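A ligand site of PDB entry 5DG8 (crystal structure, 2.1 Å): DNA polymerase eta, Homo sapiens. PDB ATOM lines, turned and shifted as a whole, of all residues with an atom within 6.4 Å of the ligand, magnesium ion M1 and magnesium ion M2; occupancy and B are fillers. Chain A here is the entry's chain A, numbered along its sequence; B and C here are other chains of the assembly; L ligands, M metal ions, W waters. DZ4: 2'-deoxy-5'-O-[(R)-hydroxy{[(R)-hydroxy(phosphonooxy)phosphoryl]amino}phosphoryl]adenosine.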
ATOM      1  N   ASP A  16     -13.255  13.666  11.231  1.00  0.00           N
ATOM      2  CA  ASP A  16     -12.525  12.409  11.244  1.00  0.00           C
ATOM      3  C   ASP A  16     -11.023  12.676  11.422  1.00  0.00           C
ATOM      4  O   ASP A  16     -10.406  13.329  10.585  1.00  0.00           O
ATOM      5  CB  ASP A  16     -12.786  11.667   9.927  1.00  0.00           C
ATOM      6  CG  ASP A  16     -12.230  10.242   9.920  1.00  0.00           C
ATOM      7  OD1 ASP A  16     -11.283   9.950  10.663  1.00  0.00           O
ATOM      8  OD2 ASP A  16     -12.739   9.431   9.133  1.00  0.00           O
ATOM      9  N   MET A  17     -10.438  12.187  12.511  1.00  0.00           N
ATOM     10  CA  MET A  17      -9.002  12.388  12.719  1.00  0.00           C
ATOM     11  C   MET A  17      -8.197  11.688  11.630  1.00  0.00           C
ATOM     12  O   MET A  17      -8.499  10.565  11.231  1.00  0.00           O
ATOM     13  CB  MET A  17      -8.540  11.881  14.097  1.00  0.00           C
ATOM     14  CG  MET A  17      -9.410  12.329  15.262  1.00  0.00           C
ATOM     15  SD  MET A  17      -9.657  14.121  15.396  1.00  0.00           S
ATOM     16  CE  MET A  17      -7.969  14.673  15.570  1.00  0.00           C
ATOM     17  N   ASP A  18      -7.207  12.400  11.093  1.00  0.00           N
ATOM     18  CA  ASP A  18      -6.282  11.834  10.139  1.00  0.00           C
ATOM     19  C   ASP A  18      -5.366  10.844  10.843  1.00  0.00           C
ATOM     20  O   ASP A  18      -4.891  11.139  11.942  1.00  0.00           O
ATOM     21  CB  ASP A  18      -5.481  12.940   9.450  1.00  0.00           C
ATOM     22  CG  ASP A  18      -6.373  13.928   8.713  1.00  0.00           C
ATOM     23  OD1 ASP A  18      -7.356  13.490   8.118  1.00  0.00           O
ATOM     24  OD2 ASP A  18      -6.078  15.138   8.742  1.00  0.00           O
ATOM     25  N   CYS A  19      -5.128   9.701  10.203  1.00  0.00           N
ATOM     26  CA  CYS A  19      -4.349   8.577  10.722  1.00  0.00           C
ATOM     27  C   CYS A  19      -4.190   8.606  12.249  1.00  0.00           C
ATOM     28  O   CYS A  19      -3.104   8.851  12.772  1.00  0.00           O
ATOM     29  CB  CYS A  19      -2.971   8.525  10.016  1.00  0.00           C
ATOM     30  SG  CYS A  19      -2.059  10.102   9.954  1.00  0.00           S
ATOM     31  N   PHE A  20      -5.297   8.405  12.945  1.00  0.00           N
ATOM     32  CA  PHE A  20      -5.420   8.876  14.327  1.00  0.00           C
ATOM     33  C   PHE A  20      -4.374   8.265  15.297  1.00  0.00           C
ATOM     34  O   PHE A  20      -3.694   9.000  16.015  1.00  0.00           O
ATOM     35  CB  PHE A  20      -6.840   8.615  14.828  1.00  0.00           C
ATOM     36  CG  PHE A  20      -7.080   9.059  16.240  1.00  0.00           C
ATOM     37  CD1 PHE A  20      -6.724  10.352  16.638  1.00  0.00           C
ATOM     38  CD2 PHE A  20      -7.605   8.198  17.169  1.00  0.00           C
ATOM     39  CE1 PHE A  20      -6.909  10.757  17.937  1.00  0.00           C
ATOM     40  CE2 PHE A  20      -7.803   8.599  18.486  1.00  0.00           C
ATOM     41  CZ  PHE A  20      -7.463   9.891  18.873  1.00  0.00           C
ATOM     42  N   PHE A  21      -4.251   6.937  15.335  1.00  0.00           N
ATOM     43  CA  PHE A  21      -3.321   6.290  16.263  1.00  0.00           C
ATOM     44  C   PHE A  21      -1.870   6.704  15.956  1.00  0.00           C
ATOM     45  O   PHE A  21      -1.069   6.878  16.868  1.00  0.00           O
ATOM     46  CB  PHE A  21      -3.426   4.770  16.203  1.00  0.00           C
ATOM     47  CG  PHE A  21      -4.660   4.201  16.822  1.00  0.00           C
ATOM     48  CD1 PHE A  21      -5.753   4.994  17.102  1.00  0.00           C
ATOM     49  CD2 PHE A  21      -4.729   2.844  17.107  1.00  0.00           C
ATOM     50  CE1 PHE A  21      -6.898   4.463  17.641  1.00  0.00           C
ATOM     51  CE2 PHE A  21      -5.880   2.306  17.657  1.00  0.00           C
ATOM     52  CZ  PHE A  21      -6.966   3.106  17.927  1.00  0.00           C
ATOM     53  N   VAL A  22      -1.541   6.871  14.681  1.00  0.00           N
ATOM     54  CA  VAL A  22      -0.223   7.378  14.297  1.00  0.00           C
ATOM     55  C   VAL A  22       0.030   8.793  14.857  1.00  0.00           C
ATOM     56  O   VAL A  22       1.109   9.063  15.390  1.00  0.00           O
ATOM     57  CB  VAL A  22      -0.061   7.367  12.743  1.00  0.00           C
ATOM     58  CG1 VAL A  22       1.099   8.197  12.306  1.00  0.00           C
ATOM     59  CG2 VAL A  22       0.125   5.947  12.248  1.00  0.00           C
ATOM     60  N   GLN A  41       0.078  -3.813  16.010  1.00  0.00           N
ATOM     61  CA  GLN A  41      -0.548  -4.533  17.096  1.00  0.00           C
ATOM     62  C   GLN A  41      -0.002  -5.942  17.140  1.00  0.00           C
ATOM     63  O   GLN A  41      -0.021  -6.627  16.122  1.00  0.00           O
ATOM     64  CB  GLN A  41      -2.053  -4.550  16.872  1.00  0.00           C
ATOM     65  CG  GLN A  41      -2.874  -4.856  18.062  1.00  0.00           C
ATOM     66  CD  GLN A  41      -4.328  -4.736  17.719  1.00  0.00           C
ATOM     67  OE1 GLN A  41      -5.100  -4.072  18.424  1.00  0.00           O
ATOM     68  NE2 GLN A  41      -4.738  -5.398  16.652  1.00  0.00           N
ATOM     69  N   ILE A  50      -0.484  -4.261  11.098  1.00  0.00           N
ATOM     70  CA  ILE A  50      -0.543  -2.817  10.907  1.00  0.00           C
ATOM     71  C   ILE A  50      -1.991  -2.339  11.033  1.00  0.00           C
ATOM     72  O   ILE A  50      -2.893  -2.909  10.417  1.00  0.00           O
ATOM     73  CB  ILE A  50      -0.001  -2.364   9.532  1.00  0.00           C
ATOM     74  CG1 ILE A  50       1.490  -2.701   9.370  1.00  0.00           C
ATOM     75  CG2 ILE A  50      -0.234  -0.873   9.343  1.00  0.00           C
ATOM     76  CD1 ILE A  50       2.370  -2.122  10.426  1.00  0.00           C
ATOM     77  N   ILE A  51      -2.224  -1.284  11.812  1.00  0.00           N
ATOM     78  CA  ILE A  51      -3.581  -0.817  12.019  1.00  0.00           C
ATOM     79  C   ILE A  51      -3.794   0.674  11.767  1.00  0.00           C
ATOM     80  O   ILE A  51      -4.916   1.159  11.787  1.00  0.00           O
ATOM     81  CB  ILE A  51      -4.043  -1.148  13.429  1.00  0.00           C
ATOM     82  CG1 ILE A  51      -3.266  -0.329  14.463  1.00  0.00           C
ATOM     83  CG2 ILE A  51      -3.867  -2.653  13.685  1.00  0.00           C
ATOM     84  CD1 ILE A  51      -3.734  -0.584  15.878  1.00  0.00           C
ATOM     85  N   ALA A  52      -2.719   1.409  11.549  1.00  0.00           N
ATOM     86  CA  ALA A  52      -2.834   2.806  11.159  1.00  0.00           C
ATOM     87  C   ALA A  52      -1.529   3.201  10.515  1.00  0.00           C
ATOM     88  O   ALA A  52      -0.494   2.666  10.875  1.00  0.00           O
ATOM     89  CB  ALA A  52      -3.158   3.709  12.365  1.00  0.00           C
ATOM     90  N   VAL A  53      -1.599   4.125   9.569  1.00  0.00           N
ATOM     91  CA  VAL A  53      -0.514   4.379   8.635  1.00  0.00           C
ATOM     92  C   VAL A  53      -0.425   5.870   8.312  1.00  0.00           C
ATOM     93  O   VAL A  53      -1.412   6.493   7.876  1.00  0.00           O
ATOM     94  CB  VAL A  53      -0.727   3.610   7.285  1.00  0.00           C
ATOM     95  CG1 VAL A  53       0.544   3.700   6.426  1.00  0.00           C
ATOM     96  CG2 VAL A  53      -1.112   2.178   7.506  1.00  0.00           C
ATOM     97  N   TYR A  55       0.591   9.234   6.233  1.00  0.00           N
ATOM     98  CA  TYR A  55       0.476   9.498   4.804  1.00  0.00           C
ATOM     99  C   TYR A  55       1.824   9.277   4.116  1.00  0.00           C
ATOM    100  O   TYR A  55       1.873   8.813   2.986  1.00  0.00           O
ATOM    101  CB  TYR A  55      -0.097  10.906   4.551  1.00  0.00           C
ATOM    102  CG  TYR A  55      -1.599  10.879   4.715  1.00  0.00           C
ATOM    103  CD1 TYR A  55      -2.173  10.858   5.969  1.00  0.00           C
ATOM    104  CD2 TYR A  55      -2.451  10.795   3.607  1.00  0.00           C
ATOM    105  CE1 TYR A  55      -3.550  10.801   6.130  1.00  0.00           C
ATOM    106  CE2 TYR A  55      -3.837  10.738   3.762  1.00  0.00           C
ATOM    107  CZ  TYR A  55      -4.377  10.734   5.019  1.00  0.00           C
ATOM    108  OH  TYR A  55      -5.746  10.678   5.185  1.00  0.00           O
ATOM    109  N   ARG A  58       1.900   5.590   3.469  1.00  0.00           N
ATOM    110  CA  ARG A  58       0.873   5.201   2.493  1.00  0.00           C
ATOM    111  C   ARG A  58       1.382   5.382   1.058  1.00  0.00           C
ATOM    112  O   ARG A  58       1.008   4.614   0.157  1.00  0.00           O
ATOM    113  CB  ARG A  58      -0.429   6.002   2.689  1.00  0.00           C
ATOM    114  CG  ARG A  58      -1.089   5.873   4.076  1.00  0.00           C
ATOM    115  CD  ARG A  58      -2.361   6.742   4.152  1.00  0.00           C
ATOM    116  NE  ARG A  58      -2.920   6.870   5.500  1.00  0.00           N
ATOM    117  CZ  ARG A  58      -4.178   7.232   5.764  1.00  0.00           C
ATOM    118  NH1 ARG A  58      -5.023   7.497   4.784  1.00  0.00           N
ATOM    119  NH2 ARG A  58      -4.599   7.324   7.018  1.00  0.00           N
ATOM    120  N   ARG A  64      -3.383  -0.525   6.322  1.00  0.00           N
ATOM    121  CA  ARG A  64      -3.823  -1.260   7.492  1.00  0.00           C
ATOM    122  C   ARG A  64      -4.160  -2.713   7.092  1.00  0.00           C
ATOM    123  O   ARG A  64      -4.320  -2.995   5.902  1.00  0.00           O
ATOM    124  CB  ARG A  64      -5.017  -0.581   8.140  1.00  0.00           C
ATOM    125  CG  ARG A  64      -6.353  -0.924   7.545  1.00  0.00           C
ATOM    126  CD  ARG A  64      -7.458  -0.153   8.271  1.00  0.00           C
ATOM    127  NE  ARG A  64      -8.032   0.881   7.418  1.00  0.00           N
ATOM    128  CZ  ARG A  64      -9.031   1.681   7.774  1.00  0.00           C
ATOM    129  NH1 ARG A  64      -9.550   1.599   8.986  1.00  0.00           N
ATOM    130  NH2 ARG A  64      -9.495   2.596   6.927  1.00  0.00           N
ATOM    131  N   SER A  65      -4.259  -3.602   8.072  1.00  0.00           N
ATOM    132  CA  SER A  65      -4.546  -5.015   7.845  1.00  0.00           C
ATOM    133  C   SER A  65      -3.449  -5.723   7.038  1.00  0.00           C
ATOM    134  O   SER A  65      -3.666  -6.767   6.439  1.00  0.00           O
ATOM    135  CB  SER A  65      -5.898  -5.198   7.139  1.00  0.00           C
ATOM    136  OG  SER A  65      -6.968  -4.903   8.019  1.00  0.00           O
ATOM    137  N   SER A 116     -17.190   6.718  16.241  1.00  0.00           N
ATOM    138  CA  SER A 116     -16.112   5.754  16.437  1.00  0.00           C
ATOM    139  C   SER A 116     -15.075   6.396  17.348  1.00  0.00           C
ATOM    140  O   SER A 116     -15.260   7.528  17.787  1.00  0.00           O
ATOM    141  CB  SER A 116     -15.462   5.357  15.113  1.00  0.00           C
ATOM    142  OG  SER A 116     -14.663   6.435  14.624  1.00  0.00           O
ATOM    143  N   ILE A 117     -13.976   5.692  17.587  1.00  0.00           N
ATOM    144  CA  ILE A 117     -12.944   6.229  18.459  1.00  0.00           C
ATOM    145  C   ILE A 117     -12.376   7.548  17.922  1.00  0.00           C
ATOM    146  O   ILE A 117     -11.922   8.370  18.719  1.00  0.00           O
ATOM    147  CB  ILE A 117     -11.797   5.194  18.665  1.00  0.00           C
ATOM    148  CG1 ILE A 117     -10.980   5.543  19.916  1.00  0.00           C
ATOM    149  CG2 ILE A 117     -10.926   5.082  17.426  1.00  0.00           C
ATOM    150  CD1 ILE A 117      -9.959   4.453  20.310  1.00  0.00           C
ATOM    151  N   ASP A 118     -12.430   7.779  16.600  1.00  0.00           N
ATOM    152  CA  ASP A 118     -11.908   9.053  16.062  1.00  0.00           C
ATOM    153  C   ASP A 118     -12.839   9.829  15.109  1.00  0.00           C
ATOM    154  O   ASP A 118     -12.378  10.647  14.331  1.00  0.00           O
ATOM    155  CB  ASP A 118     -10.581   8.793  15.335  1.00  0.00           C
ATOM    156  CG  ASP A 118     -10.767   8.304  13.912  1.00  0.00           C
ATOM    157  OD1 ASP A 118     -11.711   7.514  13.655  1.00  0.00           O
ATOM    158  OD2 ASP A 118      -9.974   8.724  13.042  1.00  0.00           O
ATOM    159  N   GLU A 119     -14.142   9.583  15.189  1.00  0.00           N
ATOM    160  CA  GLU A 119     -15.096  10.298  14.345  1.00  0.00           C
ATOM    161  C   GLU A 119     -16.275  10.785  15.178  1.00  0.00           C
ATOM    162  O   GLU A 119     -16.716  10.107  16.096  1.00  0.00           O
ATOM    163  CB  GLU A 119     -15.591   9.408  13.202  1.00  0.00           C
ATOM    164  CG  GLU A 119     -14.512   8.981  12.227  1.00  0.00           C
ATOM    165  CD  GLU A 119     -15.064   8.155  11.058  1.00  0.00           C
ATOM    166  OE1 GLU A 119     -16.272   8.191  10.804  1.00  0.00           O
ATOM    167  OE2 GLU A 119     -14.256   7.471  10.373  1.00  0.00           O
ATOM    168  N   LYS A 227     -20.273  12.653   5.792  1.00  0.00           N
ATOM    169  CA  LYS A 227     -19.278  11.584   5.867  1.00  0.00           C
ATOM    170  C   LYS A 227     -18.596  11.392   4.502  1.00  0.00           C
ATOM    171  O   LYS A 227     -17.397  11.172   4.424  1.00  0.00           O
ATOM    172  CB  LYS A 227     -19.927  10.297   6.361  1.00  0.00           C
ATOM    173  CG  LYS A 227     -19.041   9.062   6.269  1.00  0.00           C
ATOM    174  CD  LYS A 227     -18.198   8.886   7.495  1.00  0.00           C
ATOM    175  CE  LYS A 227     -17.264   7.685   7.399  1.00  0.00           C
ATOM    176  NZ  LYS A 227     -17.982   6.407   7.088  1.00  0.00           N
ATOM    177  N   LYS A 234      -8.822  14.528   2.067  1.00  0.00           N
ATOM    178  CA  LYS A 234      -7.977  14.230   3.226  1.00  0.00           C
ATOM    179  C   LYS A 234      -6.521  14.308   2.806  1.00  0.00           C
ATOM    180  O   LYS A 234      -6.216  14.069   1.642  1.00  0.00           O
ATOM    181  CB  LYS A 234      -8.292  12.838   3.787  1.00  0.00           C
ATOM    182  CG  LYS A 234      -9.621  12.727   4.537  1.00  0.00           C
ATOM    183  CD  LYS A 234      -9.860  11.287   5.042  1.00  0.00           C
ATOM    184  CE  LYS A 234      -9.071  10.926   6.287  1.00  0.00           C
ATOM    185  NZ  LYS A 234      -9.651  11.328   7.632  1.00  0.00           N
ATOM    186  N   PRO A 235      -5.598  14.638   3.744  1.00  0.00           N
ATOM    187  CA  PRO A 235      -5.740  14.969   5.178  1.00  0.00           C
ATOM    188  C   PRO A 235      -5.742  16.453   5.433  1.00  0.00           C
ATOM    189  O   PRO A 235      -5.351  17.221   4.548  1.00  0.00           O
ATOM    190  CB  PRO A 235      -4.481  14.332   5.783  1.00  0.00           C
ATOM    191  CG  PRO A 235      -3.433  14.542   4.711  1.00  0.00           C
ATOM    192  CD  PRO A 235      -4.175  14.513   3.365  1.00  0.00           C
ATOM    193  P    DT B   8     -16.461   3.115   8.048  1.00  0.00           P
ATOM    194  OP1  DT B   8     -16.501   4.319   7.184  1.00  0.00           O
ATOM    195  OP2  DT B   8     -15.913   1.839   7.546  1.00  0.00           O
ATOM    196  O5'  DT B   8     -15.599   3.365   9.382  1.00  0.00           O
ATOM    197  C5'  DT B   8     -15.988   4.341  10.324  1.00  0.00           C
ATOM    198  C4'  DT B   8     -15.144   4.184  11.582  1.00  0.00           C
ATOM    199  O4'  DT B   8     -15.377   2.875  12.143  1.00  0.00           O
ATOM    200  C3'  DT B   8     -13.630   4.277  11.362  1.00  0.00           C
ATOM    201  O3'  DT B   8     -13.004   4.938  12.466  1.00  0.00           O
ATOM    202  C2'  DT B   8     -13.210   2.819  11.273  1.00  0.00           C
ATOM    203  C1'  DT B   8     -14.160   2.188  12.279  1.00  0.00           C
ATOM    204  N1   DT B   8     -14.381   0.711  12.083  1.00  0.00           N
ATOM    205  C2   DT B   8     -14.361  -0.120  13.188  1.00  0.00           C
ATOM    206  O2   DT B   8     -14.207   0.295  14.324  1.00  0.00           O
ATOM    207  N3   DT B   8     -14.531  -1.450  12.908  1.00  0.00           N
ATOM    208  C4   DT B   8     -14.713  -2.027  11.661  1.00  0.00           C
ATOM    209  O4   DT B   8     -14.859  -3.239  11.519  1.00  0.00           O
ATOM    210  C5   DT B   8     -14.703  -1.110  10.544  1.00  0.00           C
ATOM    211  C7   DT B   8     -14.888  -1.621   9.155  1.00  0.00           C
ATOM    212  C6   DT B   8     -14.546   0.207  10.807  1.00  0.00           C
ATOM    213  P    DT C   3      -5.330 -13.151   7.473  1.00  0.00           P
ATOM    214  OP1  DT C   3      -6.184 -14.228   6.904  1.00  0.00           O
ATOM    215  OP2  DT C   3      -4.015 -12.818   6.873  1.00  0.00           O
ATOM    216  O5'  DT C   3      -6.237 -11.841   7.522  1.00  0.00           O
ATOM    217  C5'  DT C   3      -6.993 -11.581   8.671  1.00  0.00           C
ATOM    218  C4'  DT C   3      -6.239 -10.634   9.590  1.00  0.00           C
ATOM    219  O4'  DT C   3      -5.519  -9.670   8.796  1.00  0.00           O
ATOM    220  C3'  DT C   3      -7.142  -9.817  10.515  1.00  0.00           C
ATOM    221  O3'  DT C   3      -6.765 -10.033  11.840  1.00  0.00           O
ATOM    222  C2'  DT C   3      -6.939  -8.354  10.079  1.00  0.00           C
ATOM    223  C1'  DT C   3      -6.287  -8.503   8.702  1.00  0.00           C
ATOM    224  N1   DT C   3      -7.231  -8.651   7.465  1.00  0.00           N
ATOM    225  C2   DT C   3      -8.634  -8.687   7.573  1.00  0.00           C
ATOM    226  O2   DT C   3      -9.258  -8.593   8.609  1.00  0.00           O
ATOM    227  N3   DT C   3      -9.288  -8.836   6.372  1.00  0.00           N
ATOM    228  C4   DT C   3      -8.728  -8.961   5.112  1.00  0.00           C
ATOM    229  O4   DT C   3      -9.413  -9.086   4.098  1.00  0.00           O
ATOM    230  C5   DT C   3      -7.285  -8.924   5.069  1.00  0.00           C
ATOM    231  C7   DT C   3      -6.558  -9.045   3.759  1.00  0.00           C
ATOM    232  C6   DT C   3      -6.616  -8.777   6.231  1.00  0.00           C
ATOM    233  P   EDA C   4      -7.826 -10.627  12.883  1.00  0.00           P
ATOM    234  OP1 EDA C   4      -7.254 -11.842  13.534  1.00  0.00           O
ATOM    235  OP2 EDA C   4      -9.129 -10.678  12.187  1.00  0.00           O
ATOM    236  O5' EDA C   4      -7.954  -9.499  13.949  1.00  0.00           O
ATOM    237  N9  EDA C   4      -9.256  -6.020  14.702  1.00  0.00           N
ATOM    238  C4  EDA C   4      -9.626  -4.737  14.675  1.00  0.00           C
ATOM    239  N3  EDA C   4      -9.451  -3.742  15.569  1.00  0.00           N
ATOM    240  C2  EDA C   4      -9.965  -2.455  15.326  1.00  0.00           C
ATOM    241  N1  EDA C   4     -10.599  -2.316  14.080  1.00  0.00           N
ATOM    242  C6  EDA C   4     -10.764  -3.323  13.224  1.00  0.00           C
ATOM    243  C10 EDA C   4     -11.139  -1.220  13.547  1.00  0.00           C
ATOM    244  C11 EDA C   4     -11.624  -1.553  12.341  1.00  0.00           C
ATOM    245  N6  EDA C   4     -11.403  -2.854  12.144  1.00  0.00           N
ATOM    246  C5  EDA C   4     -10.297  -4.532  13.533  1.00  0.00           C
ATOM    247  N7  EDA C   4     -10.312  -5.669  12.855  1.00  0.00           N
ATOM    248  C8  EDA C   4      -9.679  -6.591  13.578  1.00  0.00           C
ATOM    249  C2' EDA C   4      -8.906  -8.037  16.242  1.00  0.00           C
ATOM    250  C5' EDA C   4      -6.982  -8.483  13.974  1.00  0.00           C
ATOM    251  C4' EDA C   4      -6.690  -8.059  15.406  1.00  0.00           C
ATOM    252  O4' EDA C   4      -7.075  -6.688  15.501  1.00  0.00           O
ATOM    253  C1' EDA C   4      -8.477  -6.616  15.851  1.00  0.00           C
ATOM    254  C3' EDA C   4      -7.569  -8.723  16.486  1.00  0.00           C
ATOM    255  O3' EDA C   4      -7.053  -8.357  17.752  1.00  0.00           O
ATOM    256  P    DA C   5      -7.790  -8.761  19.126  1.00  0.00           P
ATOM    257  OP1  DA C   5      -6.682  -8.908  20.104  1.00  0.00           O
ATOM    258  OP2  DA C   5      -8.734  -9.887  18.907  1.00  0.00           O
ATOM    259  O5'  DA C   5      -8.584  -7.450  19.508  1.00  0.00           O
ATOM    260  C5'  DA C   5      -7.868  -6.226  19.505  1.00  0.00           C
ATOM    261  C4'  DA C   5      -8.768  -5.087  19.891  1.00  0.00           C
ATOM    262  O4'  DA C   5      -9.549  -4.690  18.740  1.00  0.00           O
ATOM    263  C3'  DA C   5      -9.767  -5.403  20.986  1.00  0.00           C
ATOM    264  O3'  DA C   5      -9.849  -4.276  21.843  1.00  0.00           O
ATOM    265  C2'  DA C   5     -11.072  -5.663  20.215  1.00  0.00           C
ATOM    266  C1'  DA C   5     -10.933  -4.715  19.050  1.00  0.00           C
ATOM    267  N9   DA C   5     -11.618  -5.135  17.839  1.00  0.00           N
ATOM    268  C8   DA C   5     -11.653  -6.387  17.305  1.00  0.00           C
ATOM    269  N7   DA C   5     -12.324  -6.461  16.178  1.00  0.00           N
ATOM    270  C5   DA C   5     -12.725  -5.166  15.947  1.00  0.00           C
ATOM    271  C6   DA C   5     -13.465  -4.569  14.901  1.00  0.00           C
ATOM    272  N6   DA C   5     -13.955  -5.253  13.863  1.00  0.00           N
ATOM    273  N1   DA C   5     -13.702  -3.246  14.977  1.00  0.00           N
ATOM    274  C2   DA C   5     -13.211  -2.568  16.032  1.00  0.00           C
ATOM    275  N3   DA C   5     -12.508  -3.005  17.068  1.00  0.00           N
ATOM    276  C4   DA C   5     -12.297  -4.323  16.959  1.00  0.00           C
HETATM  277  N1  DZ4 L   1      -7.575  -2.636  12.784  1.00  0.00           N
HETATM  278  C2  DZ4 L   1      -7.174  -2.079  13.924  1.00  0.00           C
HETATM  279  N3  DZ4 L   1      -7.315  -0.768  14.198  1.00  0.00           N
HETATM  280  C4  DZ4 L   1      -7.888   0.004  13.305  1.00  0.00           C
HETATM  281  C5  DZ4 L   1      -8.305  -0.529  12.171  1.00  0.00           C
HETATM  282  C6  DZ4 L   1      -8.140  -1.890  11.881  1.00  0.00           C
HETATM  283  N6  DZ4 L   1      -8.469  -2.685  10.792  1.00  0.00           N
HETATM  284  N7  DZ4 L   1      -8.833   0.466  11.467  1.00  0.00           N
HETATM  285  C8  DZ4 L   1      -8.754   1.587  12.157  1.00  0.00           C
HETATM  286  N9  DZ4 L   1      -8.177   1.338  13.316  1.00  0.00           N
HETATM  287  PA  DZ4 L   1      -9.855   5.335  10.642  1.00  0.00           P
HETATM  288  PB  DZ4 L   1      -7.228   6.465  10.257  1.00  0.00           P
HETATM  289  PG  DZ4 L   1      -7.667   8.184   8.080  1.00  0.00           P
HETATM  290  C1' DZ4 L   1      -7.861   2.271  14.292  1.00  0.00           C
HETATM  291  O1A DZ4 L   1     -10.645   4.478   9.843  1.00  0.00           O
HETATM  292  O1B DZ4 L   1      -6.013   5.809  10.660  1.00  0.00           O
HETATM  293  O1G DZ4 L   1      -7.986   7.608   6.839  1.00  0.00           O
HETATM  294  C2' DZ4 L   1      -6.703   2.841  14.015  1.00  0.00           C
HETATM  295  O2A DZ4 L   1     -10.420   6.598  10.742  1.00  0.00           O
HETATM  296  O2B DZ4 L   1      -7.628   7.409  11.306  1.00  0.00           O
HETATM  297  O2G DZ4 L   1      -6.850   9.298   7.883  1.00  0.00           O
HETATM  298  C3' DZ4 L   1      -7.007   4.187  13.335  1.00  0.00           C
HETATM  299  O3' DZ4 L   1      -6.116   5.111  13.555  1.00  0.00           O
HETATM  300  N3A DZ4 L   1      -8.390   5.397   9.980  1.00  0.00           N
HETATM  301  O3B DZ4 L   1      -6.906   7.125   8.944  1.00  0.00           O
HETATM  302  O3G DZ4 L   1      -8.838   8.560   8.820  1.00  0.00           O
HETATM  303  C4' DZ4 L   1      -8.365   4.562  14.047  1.00  0.00           C
HETATM  304  O4' DZ4 L   1      -8.901   3.484  14.488  1.00  0.00           O
HETATM  305  C5' DZ4 L   1      -9.235   5.376  13.110  1.00  0.00           C
HETATM  306  O5' DZ4 L   1      -9.776   4.712  12.003  1.00  0.00           O
HETATM  307 MG    MG M   1      -9.529   8.692  10.878  1.00  0.00          MG
HETATM  308 MG    MG M   2     -12.701   6.839  11.769  1.00  0.00          MG
HETATM  309  O   HOH W   1      -4.267   5.047   8.974  1.00  0.00           O
HETATM  310  O   HOH W   2      -7.672   8.723   4.393  1.00  0.00           O
HETATM  311  O   HOH W   3      -8.006  -0.372  17.023  1.00  0.00           O
HETATM  312  O   HOH W   4      -6.883  -5.382  12.121  1.00  0.00           O
HETATM  313  O   HOH W   5      -6.803   2.902   9.907  1.00  0.00           O
HETATM  314  O   HOH W   6     -11.207   1.696  15.473  1.00  0.00           O
HETATM  315  O   HOH W   7     -11.301   7.726   7.703  1.00  0.00           O
HETATM  316  O   HOH W   8      -7.923   5.189   6.494  1.00  0.00           O
HETATM  317  O   HOH W   9     -11.709   3.945   7.328  1.00  0.00           O
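Water W8 bridges an oxygen (O1G) of the ligand (2.4 Å) and the guanidinium group (NH2) of Arg 64 (3.1 Å).
Water W1 lies within hydrogen-bond range of O1B of the ligand (2.5 Å), N of Val 53 (2.9 Å) and NH2 of Arg 58 (3.0 Å).
Water W2 lies within hydrogen-bond range of O1G of the ligand (2.7 Å), OH of Tyr 55 (2.9 Å) and NH1 of Arg 58 (2.9 Å).
Water W9 lies within hydrogen-bond range of the guanidinium group of Arg 64 (2.6 Å) and an oxygen (O1A) of the ligand (2.8 Å).
Water W7 lies within hydrogen-bond range of the side-chain carboxylate of Asp 16 and an oxygen (O1G) of the ligand.
Water W5 lies within hydrogen-bond range of a nitrogen (N3A) of the ligand, the guanidinium group of Arg 64 and the backbone carbonyl oxygen of Ile 51.
Magnesium ion M2 is bound by O3' of DT 8 of chain B (2.0 Å), OE2 of Glu 119 (2.2 Å), OD1 of Asp 118 (2.2 Å) and O2A of the ligand (2.5 Å).
Magnesium ion M2 has four donor atoms within binding distance.
OP1 of DT 8 of chain B is in salt-bridge range of NZ of Lys 227, at 2.6 Å.
OD2 of Asp 16 lies within salt-bridge range of NZ of Lys 234, at 3.9 Å.
OG of Ser 116 is in hydrogen-bond range of N of Glu 119, at 3.2 Å.
N of Asp 118 sits close to OG of Ser 116 (3.3 Å).
NH1 of Arg 58 sits at hydrogen-bond distance from OH of Tyr 55 (3.3 Å).
The guanidinium group of Arg 58 lies within hydrogen-bond range of the backbone carbonyl oxygen of Val 53, at 2.8 Å.
The side-chain amino group (NZ) of Lys 234 is in salt-bridge range of the side-chain carboxylate (OD1) of Asp 18.
N of Ser 65 is in hydrogen-bond range of O of Ile 50 (2.8 Å).
An oxygen (O1A) of the ligand lies within salt-bridge range of the guanidinium group (NH1) of Arg 64 (3.2 Å).
An oxygen (O2G) of the ligand sits at hydrogen-bond distance from the backbone NH of Cys 19 (2.9 Å).
The guanidinium group (NH2) of Arg 58 lies within salt-bridge range of an oxygen (O2G) of the ligand.
N of Phe 20 is in hydrogen-bond range of O3' of the ligand (3.4 Å).
An oxygen (O2G) of the ligand is in salt-bridge range of the side-chain amino group (NZ) of Lys 234 (3.5 Å).
N6 of EDA 4 of chain C lies within hydrogen-bond range of a nitrogen (N6) of the ligand, at 3.2 Å.
An oxygen (O3') of the ligand lies within hydrogen-bond range of the backbone NH (N) of Phe 21.
O2G of the ligand sits at hydrogen-bond distance from OH of Tyr 55.
Merely in contact with the ligand: Ile 51 (3.3 Å), Asp 18 (3.4 Å), Ala 52 (3.5 Å), Ser 65 (3.9 Å) and Ile 117 (3.9 Å).
Hydrophobic or aromatic side chains that line the ligand: Phe 20, Phe 21, Ile 51, Ala 52 and Ile 117.
Ser 116 touches magnesium ion M2 (OG to MG, 3.5 Å).
The nearest printed residue that does not touch magnesium ion M2 is Met 17 (5.6 Å).
Magnesium ion M1 is bound by O of Met 17.
OD1 of Asp 16 binds magnesium ion M1.
O3G of the ligand binds magnesium ion M1 (2.2 Å).
The side-chain carboxylate (OD2) of Asp 118 binds magnesium ion M1 (2.2 Å).
Magnesium ion M1 is bound by O2A of the ligand (2.3 Å).
O2B of the ligand binds magnesium ion M1.
Magnesium ion M1 has six donor atoms within binding distance.
Of the 27 residues printed, 3 come within 4 Å of magnesium ion M1.
The nearest printed residue that does not touch magnesium ion M1 is Lys 234 (4.2 Å).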
